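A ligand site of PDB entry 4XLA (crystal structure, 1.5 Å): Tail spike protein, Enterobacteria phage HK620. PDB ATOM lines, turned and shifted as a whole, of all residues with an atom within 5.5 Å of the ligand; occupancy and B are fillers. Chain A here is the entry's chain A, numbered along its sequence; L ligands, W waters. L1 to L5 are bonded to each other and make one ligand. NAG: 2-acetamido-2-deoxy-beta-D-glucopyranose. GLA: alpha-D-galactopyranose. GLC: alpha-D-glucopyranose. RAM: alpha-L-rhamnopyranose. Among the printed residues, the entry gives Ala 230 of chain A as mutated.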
ATOM      1  N   GLY A 102     -42.334  10.819 -32.200  1.00  0.00           N
ATOM      2  CA  GLY A 102     -41.144  10.025 -32.549  1.00  0.00           C
ATOM      3  C   GLY A 102     -40.265   9.781 -31.325  1.00  0.00           C
ATOM      4  O   GLY A 102     -39.360   8.926 -31.404  1.00  0.00           O
ATOM      5  N   HIS A 103     -40.536  10.416 -30.177  1.00  0.00           N
ATOM      6  CA  HIS A 103     -39.735  10.306 -28.974  1.00  0.00           C
ATOM      7  C   HIS A 103     -40.553   9.642 -27.908  1.00  0.00           C
ATOM      8  O   HIS A 103     -40.228   9.713 -26.748  1.00  0.00           O
ATOM      9  CB  HIS A 103     -39.287  11.705 -28.502  1.00  0.00           C
ATOM     10  CG  HIS A 103     -38.555  12.500 -29.522  1.00  0.00           C
ATOM     11  ND1 HIS A 103     -37.192  12.414 -29.681  1.00  0.00           N
ATOM     12  CD2 HIS A 103     -38.971  13.360 -30.472  1.00  0.00           C
ATOM     13  CE1 HIS A 103     -36.810  13.199 -30.657  1.00  0.00           C
ATOM     14  NE2 HIS A 103     -37.871  13.786 -31.160  1.00  0.00           N
ATOM     15  N   SER A 104     -41.703   9.016 -28.286  1.00  0.00           N
ATOM     16  CA  SER A 104     -42.634   8.435 -27.279  1.00  0.00           C
ATOM     17  C   SER A 104     -43.014   9.497 -26.272  1.00  0.00           C
ATOM     18  O   SER A 104     -43.286   9.213 -25.118  1.00  0.00           O
ATOM     19  CB  SER A 104     -42.029   7.231 -26.589  1.00  0.00           C
ATOM     20  OG  SER A 104     -41.618   6.341 -27.612  1.00  0.00           O
ATOM     21  N   GLN A 133     -41.374   9.274 -22.879  1.00  0.00           N
ATOM     22  CA  GLN A 133     -40.568  10.398 -22.391  1.00  0.00           C
ATOM     23  C   GLN A 133     -41.507  11.430 -21.979  1.00  0.00           C
ATOM     24  O   GLN A 133     -42.279  11.954 -22.829  1.00  0.00           O
ATOM     25  CB  GLN A 133     -39.626  10.868 -23.479  1.00  0.00           C
ATOM     26  CG  GLN A 133     -38.629   9.762 -23.879  1.00  0.00           C
ATOM     27  CD  GLN A 133     -37.477  10.296 -24.704  1.00  0.00           C
ATOM     28  OE1 GLN A 133     -36.673  11.134 -24.267  1.00  0.00           O
ATOM     29  NE2 GLN A 133     -37.301   9.770 -25.903  1.00  0.00           N
ATOM     30  N   PHE A 138     -37.921  18.551 -27.964  1.00  0.00           N
ATOM     31  CA  PHE A 138     -37.804  18.520 -29.453  1.00  0.00           C
ATOM     32  C   PHE A 138     -39.158  18.898 -30.028  1.00  0.00           C
ATOM     33  O   PHE A 138     -40.178  18.634 -29.440  1.00  0.00           O
ATOM     34  CB  PHE A 138     -37.424  17.138 -29.917  1.00  0.00           C
ATOM     35  CG  PHE A 138     -36.021  16.658 -29.454  1.00  0.00           C
ATOM     36  CD1 PHE A 138     -34.867  17.182 -30.014  1.00  0.00           C
ATOM     37  CD2 PHE A 138     -35.909  15.664 -28.515  1.00  0.00           C
ATOM     38  CE1 PHE A 138     -33.598  16.673 -29.596  1.00  0.00           C
ATOM     39  CE2 PHE A 138     -34.697  15.138 -28.123  1.00  0.00           C
ATOM     40  CZ  PHE A 138     -33.545  15.661 -28.660  1.00  0.00           C
ATOM     41  N   PRO A 143     -34.309  14.466 -34.389  1.00  0.00           N
ATOM     42  CA  PRO A 143     -33.688  15.565 -33.641  1.00  0.00           C
ATOM     43  C   PRO A 143     -32.846  16.497 -34.506  1.00  0.00           C
ATOM     44  O   PRO A 143     -32.720  17.715 -34.252  1.00  0.00           O
ATOM     45  CB  PRO A 143     -32.863  14.828 -32.596  1.00  0.00           C
ATOM     46  CG  PRO A 143     -32.772  13.429 -33.014  1.00  0.00           C
ATOM     47  CD  PRO A 143     -34.048  13.169 -33.795  1.00  0.00           C
ATOM     48  N   LEU A 173     -36.961   2.783 -24.479  1.00  0.00           N
ATOM     49  CA  LEU A 173     -36.333   3.974 -23.783  1.00  0.00           C
ATOM     50  C   LEU A 173     -37.410   4.651 -22.958  1.00  0.00           C
ATOM     51  O   LEU A 173     -38.575   4.767 -23.383  1.00  0.00           O
ATOM     52  CB  LEU A 173     -35.803   5.039 -24.787  1.00  0.00           C
ATOM     53  CG  LEU A 173     -34.656   4.498 -25.611  1.00  0.00           C
ATOM     54  CD1 LEU A 173     -34.335   5.374 -26.816  1.00  0.00           C
ATOM     55  CD2 LEU A 173     -33.421   4.108 -24.844  1.00  0.00           C
ATOM     56  N   ASN A 175     -37.727   8.214 -20.263  1.00  0.00           N
ATOM     57  CA  ASN A 175     -37.083   9.469 -19.810  1.00  0.00           C
ATOM     58  C   ASN A 175     -38.170  10.254 -19.035  1.00  0.00           C
ATOM     59  O   ASN A 175     -39.346  10.221 -19.356  1.00  0.00           O
ATOM     60  CB  ASN A 175     -36.564  10.282 -20.990  1.00  0.00           C
ATOM     61  CG  ASN A 175     -35.540  11.353 -20.619  1.00  0.00           C
ATOM     62  OD1 ASN A 175     -35.106  11.544 -19.468  1.00  0.00           O
ATOM     63  ND2 ASN A 175     -35.099  12.047 -21.652  1.00  0.00           N
ATOM     64  N   THR A 198     -34.742   4.800 -18.362  1.00  0.00           N
ATOM     65  CA  THR A 198     -33.385   4.867 -18.874  1.00  0.00           C
ATOM     66  C   THR A 198     -32.656   6.073 -18.270  1.00  0.00           C
ATOM     67  O   THR A 198     -31.494   5.956 -17.823  1.00  0.00           O
ATOM     68  CB  THR A 198     -33.410   5.022 -20.398  1.00  0.00           C
ATOM     69  OG1 THR A 198     -34.262   4.006 -20.994  1.00  0.00           O
ATOM     70  CG2 THR A 198     -32.054   4.948 -20.976  1.00  0.00           C
ATOM     71  N   TRP A 199     -33.319   7.225 -18.369  1.00  0.00           N
ATOM     72  CA  TRP A 199     -32.832   8.499 -17.777  1.00  0.00           C
ATOM     73  C   TRP A 199     -33.998   9.180 -17.012  1.00  0.00           C
ATOM     74  O   TRP A 199     -35.174   8.885 -17.323  1.00  0.00           O
ATOM     75  CB  TRP A 199     -32.395   9.465 -18.851  1.00  0.00           C
ATOM     76  CG  TRP A 199     -31.425   8.907 -19.890  1.00  0.00           C
ATOM     77  CD1 TRP A 199     -30.121   8.599 -19.729  1.00  0.00           C
ATOM     78  CD2 TRP A 199     -31.763   8.543 -21.237  1.00  0.00           C
ATOM     79  NE1 TRP A 199     -29.571   8.168 -20.906  1.00  0.00           N
ATOM     80  CE2 TRP A 199     -30.586   8.025 -21.840  1.00  0.00           C
ATOM     81  CE3 TRP A 199     -32.949   8.575 -21.962  1.00  0.00           C
ATOM     82  CZ2 TRP A 199     -30.569   7.640 -23.187  1.00  0.00           C
ATOM     83  CZ3 TRP A 199     -32.945   8.134 -23.272  1.00  0.00           C
ATOM     84  CH2 TRP A 199     -31.777   7.656 -23.856  1.00  0.00           C
ATOM     85  N   THR A 202     -32.475  14.389 -19.569  1.00  0.00           N
ATOM     86  CA  THR A 202     -31.426  14.604 -20.517  1.00  0.00           C
ATOM     87  C   THR A 202     -31.365  16.061 -20.976  1.00  0.00           C
ATOM     88  O   THR A 202     -32.415  16.727 -21.090  1.00  0.00           O
ATOM     89  CB  THR A 202     -31.547  13.745 -21.763  1.00  0.00           C
ATOM     90  OG1 THR A 202     -32.747  14.055 -22.516  1.00  0.00           O
ATOM     91  CG2 THR A 202     -31.652  12.270 -21.351  1.00  0.00           C
ATOM     92  N   LEU A 203     -30.145  16.557 -21.119  1.00  0.00           N
ATOM     93  CA  LEU A 203     -29.874  17.945 -21.471  1.00  0.00           C
ATOM     94  C   LEU A 203     -29.211  17.992 -22.801  1.00  0.00           C
ATOM     95  O   LEU A 203     -28.177  17.290 -22.970  1.00  0.00           O
ATOM     96  CB  LEU A 203     -28.969  18.641 -20.433  1.00  0.00           C
ATOM     97  CG  LEU A 203     -29.409  18.476 -18.983  1.00  0.00           C
ATOM     98  CD1 LEU A 203     -28.357  19.202 -18.120  1.00  0.00           C
ATOM     99  CD2 LEU A 203     -30.798  19.004 -18.778  1.00  0.00           C
ATOM    100  N   GLY A 204     -29.670  18.792 -23.750  1.00  0.00           N
ATOM    101  CA  GLY A 204     -28.985  18.887 -25.012  1.00  0.00           C
ATOM    102  C   GLY A 204     -29.267  17.754 -25.962  1.00  0.00           C
ATOM    103  O   GLY A 204     -29.871  16.716 -25.601  1.00  0.00           O
ATOM    104  N   TRP A 205     -28.654  17.856 -27.124  1.00  0.00           N
ATOM    105  CA  TRP A 205     -28.722  16.796 -28.135  1.00  0.00           C
ATOM    106  C   TRP A 205     -27.505  16.860 -28.961  1.00  0.00           C
ATOM    107  O   TRP A 205     -27.293  17.857 -29.709  1.00  0.00           O
ATOM    108  CB  TRP A 205     -29.968  16.822 -29.033  1.00  0.00           C
ATOM    109  CG  TRP A 205     -29.916  15.763 -30.066  1.00  0.00           C
ATOM    110  CD1 TRP A 205     -30.057  14.458 -29.866  1.00  0.00           C
ATOM    111  CD2 TRP A 205     -29.502  15.940 -31.424  1.00  0.00           C
ATOM    112  NE1 TRP A 205     -29.818  13.760 -31.035  1.00  0.00           N
ATOM    113  CE2 TRP A 205     -29.501  14.655 -32.018  1.00  0.00           C
ATOM    114  CE3 TRP A 205     -29.234  17.053 -32.209  1.00  0.00           C
ATOM    115  CZ2 TRP A 205     -29.185  14.475 -33.364  1.00  0.00           C
ATOM    116  CZ3 TRP A 205     -28.925  16.891 -33.523  1.00  0.00           C
ATOM    117  CH2 TRP A 205     -28.901  15.587 -34.098  1.00  0.00           C
ATOM    118  N   ASN A 206     -26.616  15.876 -28.809  1.00  0.00           N
ATOM    119  CA  ASN A 206     -25.370  15.814 -29.625  1.00  0.00           C
ATOM    120  C   ASN A 206     -24.596  17.079 -29.694  1.00  0.00           C
ATOM    121  O   ASN A 206     -24.124  17.502 -30.736  1.00  0.00           O
ATOM    122  CB  ASN A 206     -25.577  15.133 -30.977  1.00  0.00           C
ATOM    123  CG  ASN A 206     -26.025  13.723 -30.854  1.00  0.00           C
ATOM    124  OD1 ASN A 206     -26.117  13.149 -29.770  1.00  0.00           O
ATOM    125  ND2 ASN A 206     -26.374  13.117 -32.007  1.00  0.00           N
ATOM    126  N   ALA A 230     -30.204  -0.363 -18.977  1.00  0.00           N
ATOM    127  CA  ALA A 230     -29.201   0.563 -18.502  1.00  0.00           C
ATOM    128  C   ALA A 230     -29.890   1.783 -17.984  1.00  0.00           C
ATOM    129  O   ALA A 230     -30.933   2.215 -18.483  1.00  0.00           O
ATOM    130  CB  ALA A 230     -28.301   0.987 -19.651  1.00  0.00           C
ATOM    131  N   HIS A 231     -29.277   2.421 -17.006  1.00  0.00           N
ATOM    132  CA  HIS A 231     -29.865   3.653 -16.497  1.00  0.00           C
ATOM    133  C   HIS A 231     -28.797   4.660 -16.160  1.00  0.00           C
ATOM    134  O   HIS A 231     -27.847   4.327 -15.446  1.00  0.00           O
ATOM    135  CB  HIS A 231     -30.634   3.355 -15.241  1.00  0.00           C
ATOM    136  CG  HIS A 231     -31.106   4.577 -14.539  1.00  0.00           C
ATOM    137  ND1 HIS A 231     -32.385   5.078 -14.671  1.00  0.00           N
ATOM    138  CD2 HIS A 231     -30.465   5.410 -13.670  1.00  0.00           C
ATOM    139  CE1 HIS A 231     -32.482   6.186 -13.966  1.00  0.00           C
ATOM    140  NE2 HIS A 231     -31.335   6.398 -13.356  1.00  0.00           N
ATOM    141  N   SER A 232     -28.952   5.900 -16.637  1.00  0.00           N
ATOM    142  CA  SER A 232     -28.144   7.031 -16.144  1.00  0.00           C
ATOM    143  C   SER A 232     -29.048   8.221 -15.824  1.00  0.00           C
ATOM    144  O   SER A 232     -29.870   8.621 -16.628  1.00  0.00           O
ATOM    145  CB  SER A 232     -27.112   7.444 -17.166  1.00  0.00           C
ATOM    146  OG  SER A 232     -26.134   6.370 -17.260  1.00  0.00           O
ATOM    147  N   TYR A 235     -28.197  12.754 -18.173  1.00  0.00           N
ATOM    148  CA  TYR A 235     -27.254  12.680 -19.310  1.00  0.00           C
ATOM    149  C   TYR A 235     -27.071  14.094 -19.874  1.00  0.00           C
ATOM    150  O   TYR A 235     -28.038  14.705 -20.382  1.00  0.00           O
ATOM    151  CB  TYR A 235     -27.814  11.704 -20.338  1.00  0.00           C
ATOM    152  CG  TYR A 235     -26.887  11.164 -21.405  1.00  0.00           C
ATOM    153  CD1 TYR A 235     -26.467  11.915 -22.459  1.00  0.00           C
ATOM    154  CD2 TYR A 235     -26.465   9.828 -21.383  1.00  0.00           C
ATOM    155  CE1 TYR A 235     -25.661  11.383 -23.463  1.00  0.00           C
ATOM    156  CE2 TYR A 235     -25.697   9.310 -22.391  1.00  0.00           C
ATOM    157  CZ  TYR A 235     -25.288  10.066 -23.410  1.00  0.00           C
ATOM    158  OH  TYR A 235     -24.537   9.530 -24.420  1.00  0.00           O
ATOM    159  N   ASN A 237     -25.668  16.429 -22.444  1.00  0.00           N
ATOM    160  CA  ASN A 237     -25.237  16.320 -23.823  1.00  0.00           C
ATOM    161  C   ASN A 237     -25.255  17.692 -24.553  1.00  0.00           C
ATOM    162  O   ASN A 237     -25.405  17.804 -25.737  1.00  0.00           O
ATOM    163  CB  ASN A 237     -26.093  15.278 -24.588  1.00  0.00           C
ATOM    164  CG  ASN A 237     -25.331  14.692 -25.775  1.00  0.00           C
ATOM    165  OD1 ASN A 237     -24.144  14.909 -25.963  1.00  0.00           O
ATOM    166  ND2 ASN A 237     -26.036  13.880 -26.569  1.00  0.00           N
ATOM    167  N   CYS A 260     -26.058   4.482 -13.239  1.00  0.00           N
ATOM    168  CA  CYS A 260     -25.086   5.547 -13.123  1.00  0.00           C
ATOM    169  C   CYS A 260     -25.810   6.861 -12.775  1.00  0.00           C
ATOM    170  O   CYS A 260     -26.963   7.079 -13.270  1.00  0.00           O
ATOM    171  CB  CYS A 260     -24.324   5.699 -14.414  1.00  0.00           C
ATOM    172  SG  CYS A 260     -22.934   6.866 -14.270  1.00  0.00           S
ATOM    173  N   GLU A 263     -23.968  11.462 -16.546  1.00  0.00           N
ATOM    174  CA  GLU A 263     -23.024  11.343 -17.648  1.00  0.00           C
ATOM    175  C   GLU A 263     -22.737  12.719 -18.202  1.00  0.00           C
ATOM    176  O   GLU A 263     -23.647  13.483 -18.516  1.00  0.00           O
ATOM    177  CB  GLU A 263     -23.410  10.380 -18.759  1.00  0.00           C
ATOM    178  CG  GLU A 263     -23.843   9.009 -18.223  1.00  0.00           C
ATOM    179  CD  GLU A 263     -23.663   7.876 -19.199  1.00  0.00           C
ATOM    180  OE1 GLU A 263     -23.068   8.072 -20.269  1.00  0.00           O
ATOM    181  OE2 GLU A 263     -24.153   6.756 -18.896  1.00  0.00           O
ATOM    182  N   HIS A 265     -21.019  14.574 -21.281  1.00  0.00           N
ATOM    183  CA  HIS A 265     -20.723  14.184 -22.654  1.00  0.00           C
ATOM    184  C   HIS A 265     -20.292  15.328 -23.562  1.00  0.00           C
ATOM    185  O   HIS A 265     -20.061  15.109 -24.731  1.00  0.00           O
ATOM    186  CB  HIS A 265     -21.915  13.440 -23.250  1.00  0.00           C
ATOM    187  CG  HIS A 265     -21.958  12.008 -22.878  1.00  0.00           C
ATOM    188  ND1 HIS A 265     -21.185  11.049 -23.500  1.00  0.00           N
ATOM    189  CD2 HIS A 265     -22.688  11.362 -21.976  1.00  0.00           C
ATOM    190  CE1 HIS A 265     -21.395   9.884 -22.950  1.00  0.00           C
ATOM    191  NE2 HIS A 265     -22.265  10.051 -21.976  1.00  0.00           N
ATOM    192  N   TYR A 284     -20.081   8.877 -15.855  1.00  0.00           N
ATOM    193  CA  TYR A 284     -19.291   8.806 -17.059  1.00  0.00           C
ATOM    194  C   TYR A 284     -18.844  10.211 -17.502  1.00  0.00           C
ATOM    195  O   TYR A 284     -19.606  11.164 -17.434  1.00  0.00           O
ATOM    196  CB  TYR A 284     -20.074   8.185 -18.196  1.00  0.00           C
ATOM    197  CG  TYR A 284     -20.273   6.690 -18.094  1.00  0.00           C
ATOM    198  CD1 TYR A 284     -21.309   6.128 -17.355  1.00  0.00           C
ATOM    199  CD2 TYR A 284     -19.329   5.840 -18.641  1.00  0.00           C
ATOM    200  CE1 TYR A 284     -21.429   4.733 -17.256  1.00  0.00           C
ATOM    201  CE2 TYR A 284     -19.460   4.437 -18.562  1.00  0.00           C
ATOM    202  CZ  TYR A 284     -20.470   3.918 -17.827  1.00  0.00           C
ATOM    203  OH  TYR A 284     -20.601   2.518 -17.734  1.00  0.00           O
ATOM    204  N   VAL A 286     -17.190  11.256 -20.949  1.00  0.00           N
ATOM    205  CA  VAL A 286     -16.898  10.555 -22.233  1.00  0.00           C
ATOM    206  C   VAL A 286     -17.110  11.570 -23.368  1.00  0.00           C
ATOM    207  O   VAL A 286     -18.143  12.247 -23.412  1.00  0.00           O
ATOM    208  CB  VAL A 286     -17.825   9.346 -22.356  1.00  0.00           C
ATOM    209  CG1 VAL A 286     -17.717   8.670 -23.728  1.00  0.00           C
ATOM    210  CG2 VAL A 286     -17.488   8.313 -21.347  1.00  0.00           C
ATOM    211  N   HIS A 288     -17.969  11.059 -27.069  1.00  0.00           N
ATOM    212  CA  HIS A 288     -18.355  10.139 -28.133  1.00  0.00           C
ATOM    213  C   HIS A 288     -18.259  10.888 -29.474  1.00  0.00           C
ATOM    214  O   HIS A 288     -18.914  11.924 -29.646  1.00  0.00           O
ATOM    215  CB  HIS A 288     -19.802   9.752 -27.998  1.00  0.00           C
ATOM    216  CG  HIS A 288     -20.097   8.710 -27.006  1.00  0.00           C
ATOM    217  ND1 HIS A 288     -19.336   7.584 -26.839  1.00  0.00           N
ATOM    218  CD2 HIS A 288     -21.075   8.629 -26.070  1.00  0.00           C
ATOM    219  CE1 HIS A 288     -19.866   6.825 -25.893  1.00  0.00           C
ATOM    220  NE2 HIS A 288     -20.922   7.435 -25.415  1.00  0.00           N
ATOM    221  N   ALA A 290     -19.696  10.052 -32.006  1.00  0.00           N
ATOM    222  CA  ALA A 290     -21.066  10.074 -32.532  1.00  0.00           C
ATOM    223  C   ALA A 290     -21.905  11.258 -32.042  1.00  0.00           C
ATOM    224  O   ALA A 290     -23.026  11.496 -32.564  1.00  0.00           O
ATOM    225  CB  ALA A 290     -21.795   8.773 -32.199  1.00  0.00           C
ATOM    226  N   GLU A 291     -21.462  11.924 -30.970  1.00  0.00           N
ATOM    227  CA  GLU A 291     -22.178  13.039 -30.352  1.00  0.00           C
ATOM    228  C   GLU A 291     -21.549  14.368 -30.547  1.00  0.00           C
ATOM    229  O   GLU A 291     -21.916  15.359 -29.916  1.00  0.00           O
ATOM    230  CB  GLU A 291     -22.373  12.805 -28.831  1.00  0.00           C
ATOM    231  CG  GLU A 291     -23.235  11.562 -28.564  1.00  0.00           C
ATOM    232  CD  GLU A 291     -23.452  11.250 -27.103  1.00  0.00           C
ATOM    233  OE1 GLU A 291     -22.612  11.671 -26.294  1.00  0.00           O
ATOM    234  OE2 GLU A 291     -24.470  10.652 -26.779  1.00  0.00           O
ATOM    235  N   ASN A 362     -17.884   1.488 -26.457  1.00  0.00           N
ATOM    236  CA  ASN A 362     -19.083   0.691 -26.331  1.00  0.00           C
ATOM    237  C   ASN A 362     -18.995  -0.648 -27.034  1.00  0.00           C
ATOM    238  O   ASN A 362     -19.750  -1.541 -26.675  1.00  0.00           O
ATOM    239  CB  ASN A 362     -20.325   1.492 -26.818  1.00  0.00           C
ATOM    240  CG  ASN A 362     -20.742   2.571 -25.801  1.00  0.00           C
ATOM    241  OD1 ASN A 362     -20.267   2.581 -24.653  1.00  0.00           O
ATOM    242  ND2 ASN A 362     -21.619   3.431 -26.205  1.00  0.00           N
HETATM  243  C1  NAG L   1     -23.718   4.353 -20.818  1.00  0.00           C
HETATM  244  C2  NAG L   1     -24.754   5.166 -21.614  1.00  0.00           C
HETATM  245  C3  NAG L   1     -24.388   5.056 -23.095  1.00  0.00           C
HETATM  246  C4  NAG L   1     -23.010   5.617 -23.203  1.00  0.00           C
HETATM  247  C5  NAG L   1     -21.938   4.948 -22.247  1.00  0.00           C
HETATM  248  C6  NAG L   1     -20.654   5.744 -22.161  1.00  0.00           C
HETATM  249  C7  NAG L   1     -27.161   5.428 -20.952  1.00  0.00           C
HETATM  250  C8  NAG L   1     -28.429   4.739 -20.599  1.00  0.00           C
HETATM  251  N2  NAG L   1     -26.064   4.665 -21.324  1.00  0.00           N
HETATM  252  O1  NAG L   1     -23.992   4.392 -19.442  1.00  0.00           O
HETATM  253  O3  NAG L   1     -25.335   5.671 -23.890  1.00  0.00           O
HETATM  254  O4  NAG L   1     -22.527   5.544 -24.547  1.00  0.00           O
HETATM  255  O5  NAG L   1     -22.432   4.887 -20.956  1.00  0.00           O
HETATM  256  O6  NAG L   1     -20.853   7.092 -21.709  1.00  0.00           O
HETATM  257  O7  NAG L   1     -27.091   6.669 -20.902  1.00  0.00           O
HETATM  258  C1  GLA L   2     -25.562   5.064 -25.195  1.00  0.00           C
HETATM  259  C2  GLA L   2     -26.040   6.166 -26.149  1.00  0.00           C
HETATM  260  C3  GLA L   2     -27.441   6.675 -25.677  1.00  0.00           C
HETATM  261  C4  GLA L   2     -28.441   5.588 -25.379  1.00  0.00           C
HETATM  262  C5  GLA L   2     -27.800   4.582 -24.441  1.00  0.00           C
HETATM  263  C6  GLA L   2     -28.710   3.398 -24.110  1.00  0.00           C
HETATM  264  O2  GLA L   2     -25.044   7.169 -26.177  1.00  0.00           O
HETATM  265  O3  GLA L   2     -27.810   7.544 -26.738  1.00  0.00           O
HETATM  266  O4  GLA L   2     -28.732   4.905 -26.650  1.00  0.00           O
HETATM  267  O5  GLA L   2     -26.534   4.111 -24.909  1.00  0.00           O
HETATM  268  O6  GLA L   2     -30.007   3.914 -23.697  1.00  0.00           O
HETATM  269  C1  GLC L   3     -30.152   4.741 -26.821  1.00  0.00           C
HETATM  270  C2  GLC L   3     -30.305   3.729 -27.984  1.00  0.00           C
HETATM  271  C3  GLC L   3     -29.861   4.291 -29.311  1.00  0.00           C
HETATM  272  C4  GLC L   3     -30.588   5.579 -29.555  1.00  0.00           C
HETATM  273  C5  GLC L   3     -30.249   6.570 -28.408  1.00  0.00           C
HETATM  274  C6  GLC L   3     -30.886   7.933 -28.525  1.00  0.00           C
HETATM  275  O2  GLC L   3     -29.662   2.486 -27.693  1.00  0.00           O
HETATM  276  O3  GLC L   3     -30.256   3.307 -30.307  1.00  0.00           O
HETATM  277  O4  GLC L   3     -30.151   6.099 -30.754  1.00  0.00           O
HETATM  278  O5  GLC L   3     -30.746   5.967 -27.224  1.00  0.00           O
HETATM  279  O6  GLC L   3     -32.324   7.766 -28.645  1.00  0.00           O
HETATM  280  C1  NAG L   4     -27.697   8.972 -26.444  1.00  0.00           C
HETATM  281  C2  NAG L   4     -27.688   9.713 -27.791  1.00  0.00           C
HETATM  282  C3  NAG L   4     -27.847  11.210 -27.517  1.00  0.00           C
HETATM  283  C4  NAG L   4     -28.911  11.569 -26.484  1.00  0.00           C
HETATM  284  C5  NAG L   4     -28.662  10.767 -25.258  1.00  0.00           C
HETATM  285  C6  NAG L   4     -29.658  11.002 -24.179  1.00  0.00           C
HETATM  286  C7  NAG L   4     -26.389   8.828 -29.664  1.00  0.00           C
HETATM  287  C8  NAG L   4     -25.014   8.600 -30.238  1.00  0.00           C
HETATM  288  N2  NAG L   4     -26.454   9.442 -28.501  1.00  0.00           N
HETATM  289  O3  NAG L   4     -28.174  11.819 -28.766  1.00  0.00           O
HETATM  290  O4  NAG L   4     -28.683  12.968 -26.160  1.00  0.00           O
HETATM  291  O5  NAG L   4     -28.775   9.364 -25.574  1.00  0.00           O
HETATM  292  O6  NAG L   4     -30.976  10.692 -24.611  1.00  0.00           O
HETATM  293  O7  NAG L   4     -27.367   8.437 -30.263  1.00  0.00           O
HETATM  294  C1  RAM L   5     -32.798   8.296 -29.874  1.00  0.00           C
HETATM  295  C2  RAM L   5     -34.292   7.930 -29.942  1.00  0.00           C
HETATM  296  C3  RAM L   5     -35.123   8.826 -29.078  1.00  0.00           C
HETATM  297  C4  RAM L   5     -34.764  10.256 -29.192  1.00  0.00           C
HETATM  298  C5  RAM L   5     -33.268  10.462 -28.987  1.00  0.00           C
HETATM  299  C6  RAM L   5     -32.874  11.918 -29.158  1.00  0.00           C
HETATM  300  O2  RAM L   5     -34.698   8.236 -31.274  1.00  0.00           O
HETATM  301  O3  RAM L   5     -36.547   8.606 -29.410  1.00  0.00           O
HETATM  302  O4  RAM L   5     -35.548  10.858 -28.155  1.00  0.00           O
HETATM  303  O5  RAM L   5     -32.547   9.698 -29.989  1.00  0.00           O
HETATM  304  O   HOH W   1     -35.013  12.386 -25.962  1.00  0.00           O
HETATM  305  O   HOH W   2     -37.460   7.040 -31.171  1.00  0.00           O
HETATM  306  O   HOH W   3     -31.026   1.645 -22.683  1.00  0.00           O
HETATM  307  O   HOH W   4     -26.068   1.687 -22.018  1.00  0.00           O
HETATM  308  O   HOH W   5     -29.966  10.759 -31.008  1.00  0.00           O
HETATM  309  O   HOH W   6     -30.912  14.386 -26.616  1.00  0.00           O
HETATM  310  O   HOH W   7     -23.276   1.941 -18.493  1.00  0.00           O
HETATM  311  O   HOH W   8     -26.956   2.407 -27.165  1.00  0.00           O
HETATM  312  O   HOH W   9     -26.047   3.610 -17.762  1.00  0.00           O
HETATM  313  O   HOH W  10     -33.334  10.210 -32.852  1.00  0.00           O
HETATM  314  O   HOH W  11     -27.328  10.365 -32.532  1.00  0.00           O
HETATM  315  O   HOH W  12     -27.679   6.133 -31.412  1.00  0.00           O
HETATM  316  O   HOH W  13     -23.181   5.937 -27.883  1.00  0.00           O
HETATM  317  O   HOH W  14     -20.978   2.171 -20.861  1.00  0.00           O
HETATM  318  O   HOH W  15     -31.852   0.807 -26.942  1.00  0.00           O
HETATM  319  O   HOH W  16     -32.640  12.869 -24.874  1.00  0.00           O
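CZ of Phe 138 touches C6 of RAM L5 (3.8 Å).
Leu 173 touches the ligand.
CG2 of Thr 198 touches O6 of GLA L2, at 3.6 Å.
CG2 of Thr 202 touches O6 of NAG L4, at 3.7 Å.
Gly 204 touches the ligand.
CB of Ala 230 touches C8 of NAG L1, 3.9 Å away.
OG of Ser 232 touches O1 of NAG L1 (3.6 Å).
Tyr 284 touches the ligand.
CG2 of Val 286 touches O6 of NAG L1, 3.6 Å away.
CB of Ala 290 touches C8 of NAG L4, at 3.8 Å.
Hydrophobic or aromatic side chains within 4 Å of the ligand: His 103, Phe 138, Leu 173, Trp 199, Trp 205, Ala 230, Tyr 235, His 265, Tyr 284, Val 286, His 288 and Ala 290.
The nearest printed residue that does not touch the ligand is Pro 143 (4.1 Å).
The side-chain carboxylate (OE2) of Glu 263 lies within hydrogen-bond range of an oxygen (O1) of NAG L1 (2.4 Å).
A ring nitrogen (NE2) of His 288 lies within hydrogen-bond range of an oxygen (O4) of NAG L1.
O3 of NAG L4 is in hydrogen-bond range of OD1 of Asn 206 (2.6 Å).
O4 of RAM L5 sits at hydrogen-bond distance from ND1 of His 103 (2.7 Å).
ND2 of Asn 237 sits at hydrogen-bond distance from O4 of NAG L4 (2.8 Å).
The side-chain amide nitrogen (ND2) of Asn 362 sits at hydrogen-bond distance from an oxygen (O4) of NAG L1, at 2.8 Å.
The side-chain carboxylate (OE2) of Glu 291 sits at hydrogen-bond distance from a nitrogen (N2) of NAG L4.
An oxygen (O7) of NAG L1 is in hydrogen-bond range of the indole nitrogen (NE1) of Trp 199 (2.9 Å).
O2 of GLA L2 sits at hydrogen-bond distance from OH of Tyr 235.
The side-chain amide nitrogen (NE2) of Gln 133 sits at hydrogen-bond distance from an oxygen (O4) of RAM L5.
An oxygen (O6) of NAG L1 sits close to a ring nitrogen (NE2) of His 265 (3.3 Å).
O3 of NAG L4 sits at hydrogen-bond distance from NE1 of Trp 205.
O of Gly 102 sits at hydrogen-bond distance from O3 of RAM L5 (3.5 Å).
OE1 of Glu 263 lies within hydrogen-bond range of NE2 of His 265 (2.7 Å).
ND2 of Asn 237 sits close to N of Asn 206 (3.1 Å).
OE2 of Glu 291 is in hydrogen-bond range of OH of Tyr 235 (2.6 Å).
The side-chain carboxylate (OE1) of Glu 291 sits at hydrogen-bond distance from a ring nitrogen (ND1) of His 265, at 3.2 Å.
The side-chain hydroxyl of Tyr 235 sits close to a ring nitrogen (NE2) of His 265.
ND2 of Asn 175 lies within hydrogen-bond range of OE1 of Gln 133, 3.2 Å away.
ND1 of His 231 lies close to O of Thr 198 (3.4 Å).
The side-chain hydroxyl of Thr 202 is in hydrogen-bond range of the side-chain amide nitrogen of Asn 175.
Water W2 bridges O3 of RAM L5 and O of Gly 102.
Water W1 bridges the side-chain amide oxygen of Gln 133 and an oxygen (O4) of RAM L5.
Water W16 lies within hydrogen-bond range of OG1 of Thr 202 (2.6 Å) and O6 of NAG L4 (2.8 Å).
Water W9 lies within hydrogen-bond range of O1 of NAG L1 (2.8 Å), OG of Ser 232 (2.8 Å) and O of His 231 (3.0 Å).
Water W11 lies within hydrogen-bond range of ND2 of Asn 206 (3.0 Å) and O7 of NAG L4 (3.0 Å).
Water W14 lies within hydrogen-bond range of O5 of NAG L1 (3.1 Å) and OH of Tyr 284 (3.2 Å).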
